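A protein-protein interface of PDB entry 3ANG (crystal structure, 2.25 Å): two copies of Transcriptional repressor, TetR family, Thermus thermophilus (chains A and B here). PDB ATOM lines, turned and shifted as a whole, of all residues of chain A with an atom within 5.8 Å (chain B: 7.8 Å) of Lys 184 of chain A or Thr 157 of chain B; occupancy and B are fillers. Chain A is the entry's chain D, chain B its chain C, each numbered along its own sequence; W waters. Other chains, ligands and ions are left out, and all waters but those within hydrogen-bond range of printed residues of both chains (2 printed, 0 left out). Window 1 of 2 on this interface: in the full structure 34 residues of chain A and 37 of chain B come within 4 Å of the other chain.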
ATOM      1  N   LEU A 161     -12.308  23.311  28.686  1.00  0.00           N
ATOM      2  CA  LEU A 161     -11.602  22.459  27.735  1.00  0.00           C
ATOM      3  C   LEU A 161     -12.297  22.545  26.386  1.00  0.00           C
ATOM      4  O   LEU A 161     -11.641  22.618  25.347  1.00  0.00           O
ATOM      5  CB  LEU A 161     -11.551  20.993  28.216  1.00  0.00           C
ATOM      6  CG  LEU A 161     -10.585  20.667  29.360  1.00  0.00           C
ATOM      7  CD1 LEU A 161     -10.573  19.160  29.626  1.00  0.00           C
ATOM      8  CD2 LEU A 161      -9.180  21.144  28.986  1.00  0.00           C
ATOM      9  N   SER A 165     -10.342  23.830  23.010  1.00  0.00           N
ATOM     10  CA  SER A 165     -10.320  22.995  21.817  1.00  0.00           C
ATOM     11  C   SER A 165     -11.032  23.650  20.640  1.00  0.00           C
ATOM     12  O   SER A 165     -10.515  23.662  19.534  1.00  0.00           O
ATOM     13  CB  SER A 165     -10.975  21.636  22.098  1.00  0.00           C
ATOM     14  OG  SER A 165     -10.274  20.893  23.077  1.00  0.00           O
ATOM     15  N   ALA A 179     -14.808  16.277  16.939  1.00  0.00           N
ATOM     16  CA  ALA A 179     -15.581  15.388  17.807  1.00  0.00           C
ATOM     17  C   ALA A 179     -14.675  14.492  18.630  1.00  0.00           C
ATOM     18  O   ALA A 179     -14.915  14.271  19.816  1.00  0.00           O
ATOM     19  CB  ALA A 179     -16.562  14.519  16.976  1.00  0.00           C
ATOM     20  N   GLU A 180     -13.637  13.957  18.000  1.00  0.00           N
ATOM     21  CA  GLU A 180     -12.717  13.083  18.714  1.00  0.00           C
ATOM     22  C   GLU A 180     -11.977  13.882  19.793  1.00  0.00           C
ATOM     23  O   GLU A 180     -11.743  13.381  20.895  1.00  0.00           O
ATOM     24  CB  GLU A 180     -11.736  12.429  17.731  1.00  0.00           C
ATOM     25  CG  GLU A 180     -10.800  11.387  18.350  1.00  0.00           C
ATOM     26  CD  GLU A 180      -9.719  12.006  19.238  1.00  0.00           C
ATOM     27  OE1 GLU A 180      -9.396  13.199  19.038  1.00  0.00           O
ATOM     28  OE2 GLU A 180      -9.178  11.300  20.124  1.00  0.00           O
ATOM     29  N   GLU A 181     -11.642  15.132  19.476  1.00  0.00           N
ATOM     30  CA  GLU A 181     -10.943  16.014  20.411  1.00  0.00           C
ATOM     31  C   GLU A 181     -11.811  16.267  21.648  1.00  0.00           C
ATOM     32  O   GLU A 181     -11.319  16.243  22.776  1.00  0.00           O
ATOM     33  CB  GLU A 181     -10.574  17.329  19.687  1.00  0.00           C
ATOM     34  CG  GLU A 181     -10.126  18.519  20.551  1.00  0.00           C
ATOM     35  CD  GLU A 181      -8.699  18.405  21.083  1.00  0.00           C
ATOM     36  OE1 GLU A 181      -7.917  17.582  20.562  1.00  0.00           O
ATOM     37  OE2 GLU A 181      -8.350  19.158  22.022  1.00  0.00           O
ATOM     38  N   LEU A 182     -13.105  16.487  21.448  1.00  0.00           N
ATOM     39  CA  LEU A 182     -13.996  16.723  22.578  1.00  0.00           C
ATOM     40  C   LEU A 182     -14.188  15.426  23.356  1.00  0.00           C
ATOM     41  O   LEU A 182     -14.270  15.432  24.592  1.00  0.00           O
ATOM     42  CB  LEU A 182     -15.346  17.284  22.100  1.00  0.00           C
ATOM     43  CG  LEU A 182     -15.261  18.681  21.450  1.00  0.00           C
ATOM     44  CD1 LEU A 182     -16.653  19.161  21.007  1.00  0.00           C
ATOM     45  CD2 LEU A 182     -14.640  19.672  22.445  1.00  0.00           C
ATOM     46  N   GLU A 183     -14.240  14.314  22.632  1.00  0.00           N
ATOM     47  CA  GLU A 183     -14.401  13.004  23.262  1.00  0.00           C
ATOM     48  C   GLU A 183     -13.157  12.775  24.143  1.00  0.00           C
ATOM     49  O   GLU A 183     -13.231  12.160  25.217  1.00  0.00           O
ATOM     50  CB  GLU A 183     -14.524  11.915  22.184  1.00  0.00           C
ATOM     51  CG  GLU A 183     -15.193  10.617  22.625  1.00  0.00           C
ATOM     52  CD  GLU A 183     -16.700  10.744  22.870  1.00  0.00           C
ATOM     53  OE1 GLU A 183     -17.106  11.435  23.827  1.00  0.00           O
ATOM     54  OE2 GLU A 183     -17.486  10.145  22.108  1.00  0.00           O
ATOM     55  N   LYS A 184     -12.012  13.284  23.682  1.00  0.00           N
ATOM     56  CA  LYS A 184     -10.755  13.159  24.431  1.00  0.00           C
ATOM     57  C   LYS A 184     -10.841  13.964  25.738  1.00  0.00           C
ATOM     58  O   LYS A 184     -10.440  13.483  26.807  1.00  0.00           O
ATOM     59  CB  LYS A 184      -9.574  13.665  23.587  1.00  0.00           C
ATOM     60  CG  LYS A 184      -8.285  13.885  24.360  1.00  0.00           C
ATOM     61  CD  LYS A 184      -7.586  15.190  23.942  1.00  0.00           C
ATOM     62  CE  LYS A 184      -7.923  16.341  24.878  1.00  0.00           C
ATOM     63  NZ  LYS A 184      -7.376  17.669  24.419  1.00  0.00           N
ATOM     64  N   ASN A 185     -11.359  15.190  25.652  1.00  0.00           N
ATOM     65  CA  ASN A 185     -11.486  16.026  26.837  1.00  0.00           C
ATOM     66  C   ASN A 185     -12.349  15.344  27.887  1.00  0.00           C
ATOM     67  O   ASN A 185     -11.980  15.276  29.055  1.00  0.00           O
ATOM     68  CB  ASN A 185     -12.099  17.384  26.498  1.00  0.00           C
ATOM     69  CG  ASN A 185     -11.199  18.232  25.622  1.00  0.00           C
ATOM     70  OD1 ASN A 185      -9.980  18.026  25.579  1.00  0.00           O
ATOM     71  ND2 ASN A 185     -11.794  19.213  24.926  1.00  0.00           N
ATOM     72  N   LEU A 186     -13.508  14.854  27.464  1.00  0.00           N
ATOM     73  CA  LEU A 186     -14.452  14.180  28.353  1.00  0.00           C
ATOM     74  C   LEU A 186     -13.787  13.010  29.056  1.00  0.00           C
ATOM     75  O   LEU A 186     -13.839  12.883  30.271  1.00  0.00           O
ATOM     76  CB  LEU A 186     -15.658  13.674  27.552  1.00  0.00           C
ATOM     77  CG  LEU A 186     -16.594  12.698  28.268  1.00  0.00           C
ATOM     78  CD1 LEU A 186     -17.101  13.342  29.555  1.00  0.00           C
ATOM     79  CD2 LEU A 186     -17.762  12.356  27.368  1.00  0.00           C
ATOM     80  N   ARG A 187     -13.137  12.173  28.263  1.00  0.00           N
ATOM     81  CA  ARG A 187     -12.452  10.984  28.750  1.00  0.00           C
ATOM     82  C   ARG A 187     -11.334  11.262  29.761  1.00  0.00           C
ATOM     83  O   ARG A 187     -11.228  10.578  30.792  1.00  0.00           O
ATOM     84  CB  ARG A 187     -11.893  10.208  27.555  1.00  0.00           C
ATOM     85  CG  ARG A 187     -12.263   8.744  27.542  1.00  0.00           C
ATOM     86  CD  ARG A 187     -12.760   8.327  26.169  1.00  0.00           C
ATOM     87  NE  ARG A 187     -14.203   8.504  26.042  1.00  0.00           N
ATOM     88  CZ  ARG A 187     -14.896   8.236  24.937  1.00  0.00           C
ATOM     89  NH1 ARG A 187     -14.275   7.785  23.854  1.00  0.00           N
ATOM     90  NH2 ARG A 187     -16.215   8.405  24.918  1.00  0.00           N
ATOM     91  N   LEU A 188     -10.499  12.255  29.464  1.00  0.00           N
ATOM     92  CA  LEU A 188      -9.409  12.594  30.366  1.00  0.00           C
ATOM     93  C   LEU A 188      -9.927  13.159  31.676  1.00  0.00           C
ATOM     94  O   LEU A 188      -9.428  12.829  32.748  1.00  0.00           O
ATOM     95  CB  LEU A 188      -8.461  13.623  29.728  1.00  0.00           C
ATOM     96  CG  LEU A 188      -7.614  13.185  28.536  1.00  0.00           C
ATOM     97  CD1 LEU A 188      -6.385  14.113  28.407  1.00  0.00           C
ATOM     98  CD2 LEU A 188      -7.150  11.752  28.763  1.00  0.00           C
ATOM     99  N   LEU A 189     -10.939  14.000  31.599  1.00  0.00           N
ATOM    100  CA  LEU A 189     -11.458  14.629  32.807  1.00  0.00           C
ATOM    101  C   LEU A 189     -12.357  13.719  33.662  1.00  0.00           C
ATOM    102  O   LEU A 189     -12.334  13.780  34.894  1.00  0.00           O
ATOM    103  CB  LEU A 189     -12.193  15.918  32.428  1.00  0.00           C
ATOM    104  CG  LEU A 189     -12.205  17.019  33.494  1.00  0.00           C
ATOM    105  CD1 LEU A 189     -10.778  17.486  33.793  1.00  0.00           C
ATOM    106  CD2 LEU A 189     -13.038  18.187  32.975  1.00  0.00           C
ATOM    107  N   PHE B  90       3.671  22.733  38.903  1.00  0.00           N
ATOM    108  CA  PHE B  90       2.535  23.641  38.925  1.00  0.00           C
ATOM    109  C   PHE B  90       2.576  24.608  40.071  1.00  0.00           C
ATOM    110  O   PHE B  90       2.080  25.726  39.968  1.00  0.00           O
ATOM    111  CB  PHE B  90       1.225  22.861  38.865  1.00  0.00           C
ATOM    112  CG  PHE B  90       0.968  22.298  37.506  1.00  0.00           C
ATOM    113  CD1 PHE B  90       1.326  20.994  37.196  1.00  0.00           C
ATOM    114  CD2 PHE B  90       0.493  23.121  36.486  1.00  0.00           C
ATOM    115  CE1 PHE B  90       1.222  20.517  35.893  1.00  0.00           C
ATOM    116  CE2 PHE B  90       0.388  22.645  35.179  1.00  0.00           C
ATOM    117  CZ  PHE B  90       0.755  21.346  34.890  1.00  0.00           C
ATOM    118  N   GLY B 129       3.516  22.224  27.194  1.00  0.00           N
ATOM    119  CA  GLY B 129       2.918  20.945  26.888  1.00  0.00           C
ATOM    120  C   GLY B 129       3.938  19.832  26.779  1.00  0.00           C
ATOM    121  O   GLY B 129       3.729  18.746  27.342  1.00  0.00           O
ATOM    122  N   ILE B 132       5.604  18.930  30.195  1.00  0.00           N
ATOM    123  CA  ILE B 132       4.715  18.074  30.968  1.00  0.00           C
ATOM    124  C   ILE B 132       4.811  16.643  30.438  1.00  0.00           C
ATOM    125  O   ILE B 132       4.911  15.702  31.218  1.00  0.00           O
ATOM    126  CB  ILE B 132       3.243  18.548  30.880  1.00  0.00           C
ATOM    127  CG1 ILE B 132       3.107  19.909  31.567  1.00  0.00           C
ATOM    128  CG2 ILE B 132       2.307  17.494  31.511  1.00  0.00           C
ATOM    129  CD1 ILE B 132       1.713  20.521  31.474  1.00  0.00           C
ATOM    130  N   ARG B 146      -2.698   5.745  31.054  1.00  0.00           N
ATOM    131  CA  ARG B 146      -3.406   5.223  29.889  1.00  0.00           C
ATOM    132  C   ARG B 146      -2.568   5.394  28.624  1.00  0.00           C
ATOM    133  O   ARG B 146      -1.636   6.211  28.583  1.00  0.00           O
ATOM    134  CB  ARG B 146      -4.778   5.889  29.729  1.00  0.00           C
ATOM    135  CG  ARG B 146      -4.759   7.372  29.446  1.00  0.00           C
ATOM    136  CD  ARG B 146      -6.118   7.978  29.760  1.00  0.00           C
ATOM    137  NE  ARG B 146      -7.180   7.324  29.001  1.00  0.00           N
ATOM    138  CZ  ARG B 146      -8.481   7.460  29.245  1.00  0.00           C
ATOM    139  NH1 ARG B 146      -8.906   8.234  30.238  1.00  0.00           N
ATOM    140  NH2 ARG B 146      -9.361   6.818  28.489  1.00  0.00           N
ATOM    141  N   ASP B 148      -4.282   5.237  25.334  1.00  0.00           N
ATOM    142  CA  ASP B 148      -5.196   5.471  24.227  1.00  0.00           C
ATOM    143  C   ASP B 148      -5.090   6.925  23.767  1.00  0.00           C
ATOM    144  O   ASP B 148      -5.798   7.371  22.860  1.00  0.00           O
ATOM    145  CB  ASP B 148      -6.630   5.107  24.634  1.00  0.00           C
ATOM    146  CG  ASP B 148      -7.045   5.722  25.957  1.00  0.00           C
ATOM    147  OD1 ASP B 148      -6.163   6.069  26.775  1.00  0.00           O
ATOM    148  OD2 ASP B 148      -8.268   5.838  26.187  1.00  0.00           O
ATOM    149  N   PHE B 149      -4.185   7.657  24.406  1.00  0.00           N
ATOM    150  CA  PHE B 149      -3.914   9.053  24.056  1.00  0.00           C
ATOM    151  C   PHE B 149      -2.406   9.204  24.202  1.00  0.00           C
ATOM    152  O   PHE B 149      -1.804   8.622  25.104  1.00  0.00           O
ATOM    153  CB  PHE B 149      -4.665  10.022  24.989  1.00  0.00           C
ATOM    154  CG  PHE B 149      -6.154   9.996  24.806  1.00  0.00           C
ATOM    155  CD1 PHE B 149      -6.722  10.346  23.583  1.00  0.00           C
ATOM    156  CD2 PHE B 149      -6.987   9.579  25.833  1.00  0.00           C
ATOM    157  CE1 PHE B 149      -8.097  10.273  23.385  1.00  0.00           C
ATOM    158  CE2 PHE B 149      -8.359   9.506  25.648  1.00  0.00           C
ATOM    159  CZ  PHE B 149      -8.916   9.852  24.420  1.00  0.00           C
ATOM    160  N   SER B 150      -1.789   9.963  23.309  1.00  0.00           N
ATOM    161  CA  SER B 150      -0.342  10.127  23.352  1.00  0.00           C
ATOM    162  C   SER B 150       0.104  11.040  24.483  1.00  0.00           C
ATOM    163  O   SER B 150      -0.660  11.871  24.962  1.00  0.00           O
ATOM    164  CB  SER B 150       0.166  10.687  22.019  1.00  0.00           C
ATOM    165  OG  SER B 150      -0.285  12.016  21.826  1.00  0.00           O
ATOM    166  N   LEU B 151       1.343  10.864  24.917  1.00  0.00           N
ATOM    167  CA  LEU B 151       1.900  11.698  25.968  1.00  0.00           C
ATOM    168  C   LEU B 151       1.782  13.160  25.534  1.00  0.00           C
ATOM    169  O   LEU B 151       1.426  14.028  26.333  1.00  0.00           O
ATOM    170  CB  LEU B 151       3.372  11.357  26.181  1.00  0.00           C
ATOM    171  CG  LEU B 151       3.660   9.966  26.742  1.00  0.00           C
ATOM    172  CD1 LEU B 151       5.172   9.768  26.868  1.00  0.00           C
ATOM    173  CD2 LEU B 151       2.978   9.819  28.101  1.00  0.00           C
ATOM    174  N   GLU B 152       2.071  13.422  24.261  1.00  0.00           N
ATOM    175  CA  GLU B 152       2.013  14.777  23.742  1.00  0.00           C
ATOM    176  C   GLU B 152       0.648  15.437  23.886  1.00  0.00           C
ATOM    177  O   GLU B 152       0.562  16.567  24.351  1.00  0.00           O
ATOM    178  CB  GLU B 152       2.443  14.832  22.270  1.00  0.00           C
ATOM    179  CG  GLU B 152       2.198  16.211  21.675  1.00  0.00           C
ATOM    180  CD  GLU B 152       2.916  16.466  20.360  1.00  0.00           C
ATOM    181  OE1 GLU B 152       2.652  15.737  19.373  1.00  0.00           O
ATOM    182  OE2 GLU B 152       3.738  17.414  20.319  1.00  0.00           O
ATOM    183  N   ARG B 153      -0.416  14.747  23.484  1.00  0.00           N
ATOM    184  CA  ARG B 153      -1.742  15.342  23.581  1.00  0.00           C
ATOM    185  C   ARG B 153      -2.190  15.533  25.018  1.00  0.00           C
ATOM    186  O   ARG B 153      -2.937  16.467  25.309  1.00  0.00           O
ATOM    187  CB  ARG B 153      -2.786  14.514  22.822  1.00  0.00           C
ATOM    188  CG  ARG B 153      -2.711  14.643  21.304  1.00  0.00           C
ATOM    189  CD  ARG B 153      -3.837  13.868  20.628  1.00  0.00           C
ATOM    190  NE  ARG B 153      -5.133  14.523  20.763  1.00  0.00           N
ATOM    191  CZ  ARG B 153      -6.297  13.892  20.616  1.00  0.00           C
ATOM    192  NH1 ARG B 153      -6.322  12.589  20.339  1.00  0.00           N
ATOM    193  NH2 ARG B 153      -7.439  14.558  20.722  1.00  0.00           N
ATOM    194  N   MET B 154      -1.745  14.657  25.917  1.00  0.00           N
ATOM    195  CA  MET B 154      -2.132  14.781  27.323  1.00  0.00           C
ATOM    196  C   MET B 154      -1.404  15.953  27.960  1.00  0.00           C
ATOM    197  O   MET B 154      -2.018  16.769  28.639  1.00  0.00           O
ATOM    198  CB  MET B 154      -1.853  13.481  28.096  1.00  0.00           C
ATOM    199  CG  MET B 154      -2.690  12.308  27.587  1.00  0.00           C
ATOM    200  SD  MET B 154      -2.765  10.673  28.663  1.00  0.00           S
ATOM    201  CE  MET B 154      -4.551  10.194  28.182  1.00  0.00           C
ATOM    202  N   GLY B 155      -0.094  16.036  27.739  1.00  0.00           N
ATOM    203  CA  GLY B 155       0.670  17.150  28.283  1.00  0.00           C
ATOM    204  C   GLY B 155       0.106  18.466  27.762  1.00  0.00           C
ATOM    205  O   GLY B 155      -0.054  19.419  28.518  1.00  0.00           O
ATOM    206  N   ARG B 156      -0.215  18.514  26.469  1.00  0.00           N
ATOM    207  CA  ARG B 156      -0.775  19.723  25.861  1.00  0.00           C
ATOM    208  C   ARG B 156      -2.103  20.113  26.523  1.00  0.00           C
ATOM    209  O   ARG B 156      -2.393  21.299  26.712  1.00  0.00           O
ATOM    210  CB  ARG B 156      -1.013  19.526  24.354  1.00  0.00           C
ATOM    211  CG  ARG B 156      -1.867  20.657  23.743  1.00  0.00           C
ATOM    212  CD  ARG B 156      -2.109  20.494  22.257  1.00  0.00           C
ATOM    213  NE  ARG B 156      -0.854  20.466  21.516  1.00  0.00           N
ATOM    214  CZ  ARG B 156      -0.768  20.348  20.192  1.00  0.00           C
ATOM    215  NH1 ARG B 156       0.418  20.329  19.598  1.00  0.00           N
ATOM    216  NH2 ARG B 156      -1.872  20.256  19.458  1.00  0.00           N
ATOM    217  N   THR B 157      -2.916  19.114  26.853  1.00  0.00           N
ATOM    218  CA  THR B 157      -4.200  19.359  27.504  1.00  0.00           C
ATOM    219  C   THR B 157      -3.965  19.972  28.886  1.00  0.00           C
ATOM    220  O   THR B 157      -4.646  20.910  29.277  1.00  0.00           O
ATOM    221  CB  THR B 157      -5.003  18.047  27.659  1.00  0.00           C
ATOM    222  OG1 THR B 157      -5.321  17.529  26.356  1.00  0.00           O
ATOM    223  CG2 THR B 157      -6.287  18.295  28.453  1.00  0.00           C
ATOM    224  N   LEU B 158      -2.993  19.454  29.623  1.00  0.00           N
ATOM    225  CA  LEU B 158      -2.724  20.021  30.931  1.00  0.00           C
ATOM    226  C   LEU B 158      -2.163  21.441  30.765  1.00  0.00           C
ATOM    227  O   LEU B 158      -2.530  22.342  31.517  1.00  0.00           O
ATOM    228  CB  LEU B 158      -1.746  19.141  31.707  1.00  0.00           C
ATOM    229  CG  LEU B 158      -1.629  19.495  33.192  1.00  0.00           C
ATOM    230  CD1 LEU B 158      -3.030  19.761  33.799  1.00  0.00           C
ATOM    231  CD2 LEU B 158      -0.933  18.349  33.918  1.00  0.00           C
ATOM    232  N   ALA B 159      -1.292  21.647  29.769  1.00  0.00           N
ATOM    233  CA  ALA B 159      -0.709  22.978  29.526  1.00  0.00           C
ATOM    234  C   ALA B 159      -1.807  23.975  29.140  1.00  0.00           C
ATOM    235  O   ALA B 159      -1.766  25.157  29.535  1.00  0.00           O
ATOM    236  CB  ALA B 159       0.353  22.905  28.433  1.00  0.00           C
ATOM    237  N   ASP B 160      -2.809  23.502  28.397  1.00  0.00           N
ATOM    238  CA  ASP B 160      -3.906  24.386  28.005  1.00  0.00           C
ATOM    239  C   ASP B 160      -4.702  24.842  29.227  1.00  0.00           C
ATOM    240  O   ASP B 160      -5.152  25.987  29.292  1.00  0.00           O
ATOM    241  CB  ASP B 160      -4.841  23.692  27.014  1.00  0.00           C
ATOM    242  CG  ASP B 160      -4.186  23.456  25.662  1.00  0.00           C
ATOM    243  OD1 ASP B 160      -3.442  24.348  25.190  1.00  0.00           O
ATOM    244  OD2 ASP B 160      -4.422  22.391  25.064  1.00  0.00           O
ATOM    245  N   LEU B 161      -4.884  23.941  30.192  1.00  0.00           N
ATOM    246  CA  LEU B 161      -5.616  24.280  31.419  1.00  0.00           C
ATOM    247  C   LEU B 161      -4.825  25.342  32.190  1.00  0.00           C
ATOM    248  O   LEU B 161      -5.380  26.334  32.664  1.00  0.00           O
ATOM    249  CB  LEU B 161      -5.838  23.032  32.305  1.00  0.00           C
ATOM    250  CG  LEU B 161      -7.015  22.127  31.924  1.00  0.00           C
ATOM    251  CD1 LEU B 161      -7.376  21.220  33.099  1.00  0.00           C
ATOM    252  CD2 LEU B 161      -8.226  22.975  31.581  1.00  0.00           C
ATOM    253  N   TYR B 162      -3.520  25.128  32.301  1.00  0.00           N
ATOM    254  CA  TYR B 162      -2.683  26.087  32.990  1.00  0.00           C
ATOM    255  C   TYR B 162      -2.863  27.455  32.332  1.00  0.00           C
ATOM    256  O   TYR B 162      -3.128  28.458  33.013  1.00  0.00           O
ATOM    257  CB  TYR B 162      -1.210  25.691  32.907  1.00  0.00           C
ATOM    258  CG  TYR B 162      -0.332  26.892  33.122  1.00  0.00           C
ATOM    259  CD1 TYR B 162      -0.195  27.462  34.394  1.00  0.00           C
ATOM    260  CD2 TYR B 162       0.254  27.546  32.036  1.00  0.00           C
ATOM    261  CE1 TYR B 162       0.491  28.660  34.569  1.00  0.00           C
ATOM    262  CE2 TYR B 162       0.941  28.738  32.196  1.00  0.00           C
ATOM    263  CZ  TYR B 162       1.054  29.298  33.462  1.00  0.00           C
ATOM    264  OH  TYR B 162       1.670  30.524  33.608  1.00  0.00           O
ATOM    265  N   PHE B 163      -2.730  27.484  31.005  1.00  0.00           N
ATOM    266  CA  PHE B 163      -2.862  28.729  30.255  1.00  0.00           C
ATOM    267  C   PHE B 163      -4.190  29.430  30.566  1.00  0.00           C
ATOM    268  O   PHE B 163      -4.212  30.604  30.960  1.00  0.00           O
ATOM    269  CB  PHE B 163      -2.736  28.466  28.742  1.00  0.00           C
ATOM    270  CG  PHE B 163      -3.139  29.643  27.892  1.00  0.00           C
ATOM    271  CD1 PHE B 163      -2.271  30.719  27.703  1.00  0.00           C
ATOM    272  CD2 PHE B 163      -4.425  29.716  27.349  1.00  0.00           C
ATOM    273  CE1 PHE B 163      -2.683  31.851  26.994  1.00  0.00           C
ATOM    274  CE2 PHE B 163      -4.842  30.836  26.642  1.00  0.00           C
ATOM    275  CZ  PHE B 163      -3.977  31.905  26.465  1.00  0.00           C
ATOM    276  N   ASN B 185      -6.541  21.586  38.545  1.00  0.00           N
ATOM    277  CA  ASN B 185      -6.438  21.121  37.167  1.00  0.00           C
ATOM    278  C   ASN B 185      -5.617  19.851  37.106  1.00  0.00           C
ATOM    279  O   ASN B 185      -5.955  18.909  36.390  1.00  0.00           O
ATOM    280  CB  ASN B 185      -5.782  22.169  36.270  1.00  0.00           C
ATOM    281  CG  ASN B 185      -6.587  23.443  36.176  1.00  0.00           C
ATOM    282  OD1 ASN B 185      -7.826  23.420  36.177  1.00  0.00           O
ATOM    283  ND2 ASN B 185      -5.889  24.569  36.069  1.00  0.00           N
ATOM    284  N   LEU B 189      -7.257  16.236  35.897  1.00  0.00           N
ATOM    285  CA  LEU B 189      -6.825  15.601  34.672  1.00  0.00           C
ATOM    286  C   LEU B 189      -6.031  14.337  34.976  1.00  0.00           C
ATOM    287  O   LEU B 189      -6.066  13.370  34.212  1.00  0.00           O
ATOM    288  CB  LEU B 189      -5.978  16.567  33.833  1.00  0.00           C
ATOM    289  CG  LEU B 189      -5.870  16.166  32.355  1.00  0.00           C
ATOM    290  CD1 LEU B 189      -7.254  16.246  31.713  1.00  0.00           C
ATOM    291  CD2 LEU B 189      -4.888  17.077  31.614  1.00  0.00           C
HETATM  292  O   HOH W   1      -4.428  17.975  23.337  1.00  0.00           O
HETATM  293  O   HOH W   2      -5.423  17.216  20.804  1.00  0.00           O
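OG of Ser 150 of chain B sits at hydrogen-bond distance from N of Arg 153 of chain B. The side-chain amino group (NZ) of Lys 184 of chain A lies within salt-bridge range of the side-chain carboxylate (OE2) of Glu 181 of chain A (3.0 Å). The guanidinium group of Arg 146 of chain B is in salt-bridge range of the side-chain carboxylate of Asp 148 of chain B (2.7 Å). The side-chain hydroxyl of Ser 165 of chain A sits at hydrogen-bond distance from the side-chain carboxylate of Glu 181 of chain A. The side-chain amide oxygen (OD1) of Asn 185 of chain A sits close to the side-chain amino group (NZ) of Lys 184 of chain A. O of Leu 161 of chain A sits at hydrogen-bond distance from OG of Ser 165 of chain A.
Of chain B, only Phe 149 (3.7 Å), Arg 153 (3.3 Å) and Thr 157 (2.8 Å) come within 4 Å of Lys 184 of chain A. Thr 157 of chain B touches one residue of chain A. Printed residues of chain B within 4 Å of Arg 187 of chain A: Arg 146. Of the printed residues of chain A, Leu 161 of chain B touches Leu 161 (3.3 Å). Of the printed residues of chain A, Arg 153 of chain B touches Glu 180 (2.9 Å), Glu 181 (3.1 Å) and Lys 184 (3.3 Å). Asn 185 of chain A touches none of the printed residues of chain B. Ser 165 of chain A touches none of the printed residues of chain B. The nearest residue of chain B that does not touch Lys 184 of chain A is Asp 160 of chain B (5.6 Å).
Leu 161 of chain B touches its own counterpart, Leu 161 of chain A. 3 positions are printed for both chains.
O of Arg 187 of chain A lies within hydrogen-bond range of NH1 of Arg 146 of chain B, 3.3 Å away. NZ of Lys 184 of chain A is in hydrogen-bond range of OG1 of Thr 157 of chain B (2.8 Å). NH2 of Arg 153 of chain B is in salt-bridge range of OE1 of Glu 181 of chain A (3.1 Å). NH2 of Arg 153 of chain B is in salt-bridge range of OE1 of Glu 180 of chain A, at 2.9 Å.
Hydrophobic or aromatic side chains of chain A that line the printed part of chain B: Leu 161 and Leu 188. Of the 22 printed residues of chain B, 7 touch a printed residue of chain A. Printed residues of chain B that touch a printed residue of chain A: Arg 146, Phe 149, Arg 153, Met 154, Thr 157, Leu 161 and Leu 189. Among the printed residues, Asp or Glu carboxylates within 4 Å of a Lys or Arg side-chain nitrogen of the other chain: Glu 180 of chain A with Arg 153 of chain B and Glu 181 of chain A with Arg 153 of chain B.
Water W2 bridges the side-chain carboxylate of Glu 181 of chain A (2.5 Å) and the guanidinium group of Arg 153 of chain B (2.7 Å). Water W1 lies within hydrogen-bond range of O of Arg 153 of chain B, NZ of Lys 184 of chain A and OG1 of Thr 157 of chain B.
Among the printed residues, merely in contact across the chains: Leu 188 of chain A with Met 154 of chain B (3.1 Å), Lys 184 of chain A with Arg 153 of chain B (3.3 Å), Leu 161 of chain A with Leu 161 of chain B (3.3 Å), Leu 188 of chain A with Leu 189 of chain B (3.5 Å), Glu 180 of chain A with Phe 149 of chain B (3.6 Å), Leu 188 of chain A with Phe 149 of chain B (3.7 Å) and Lys 184 of chain A with Phe 149 of chain B (3.7 Å).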
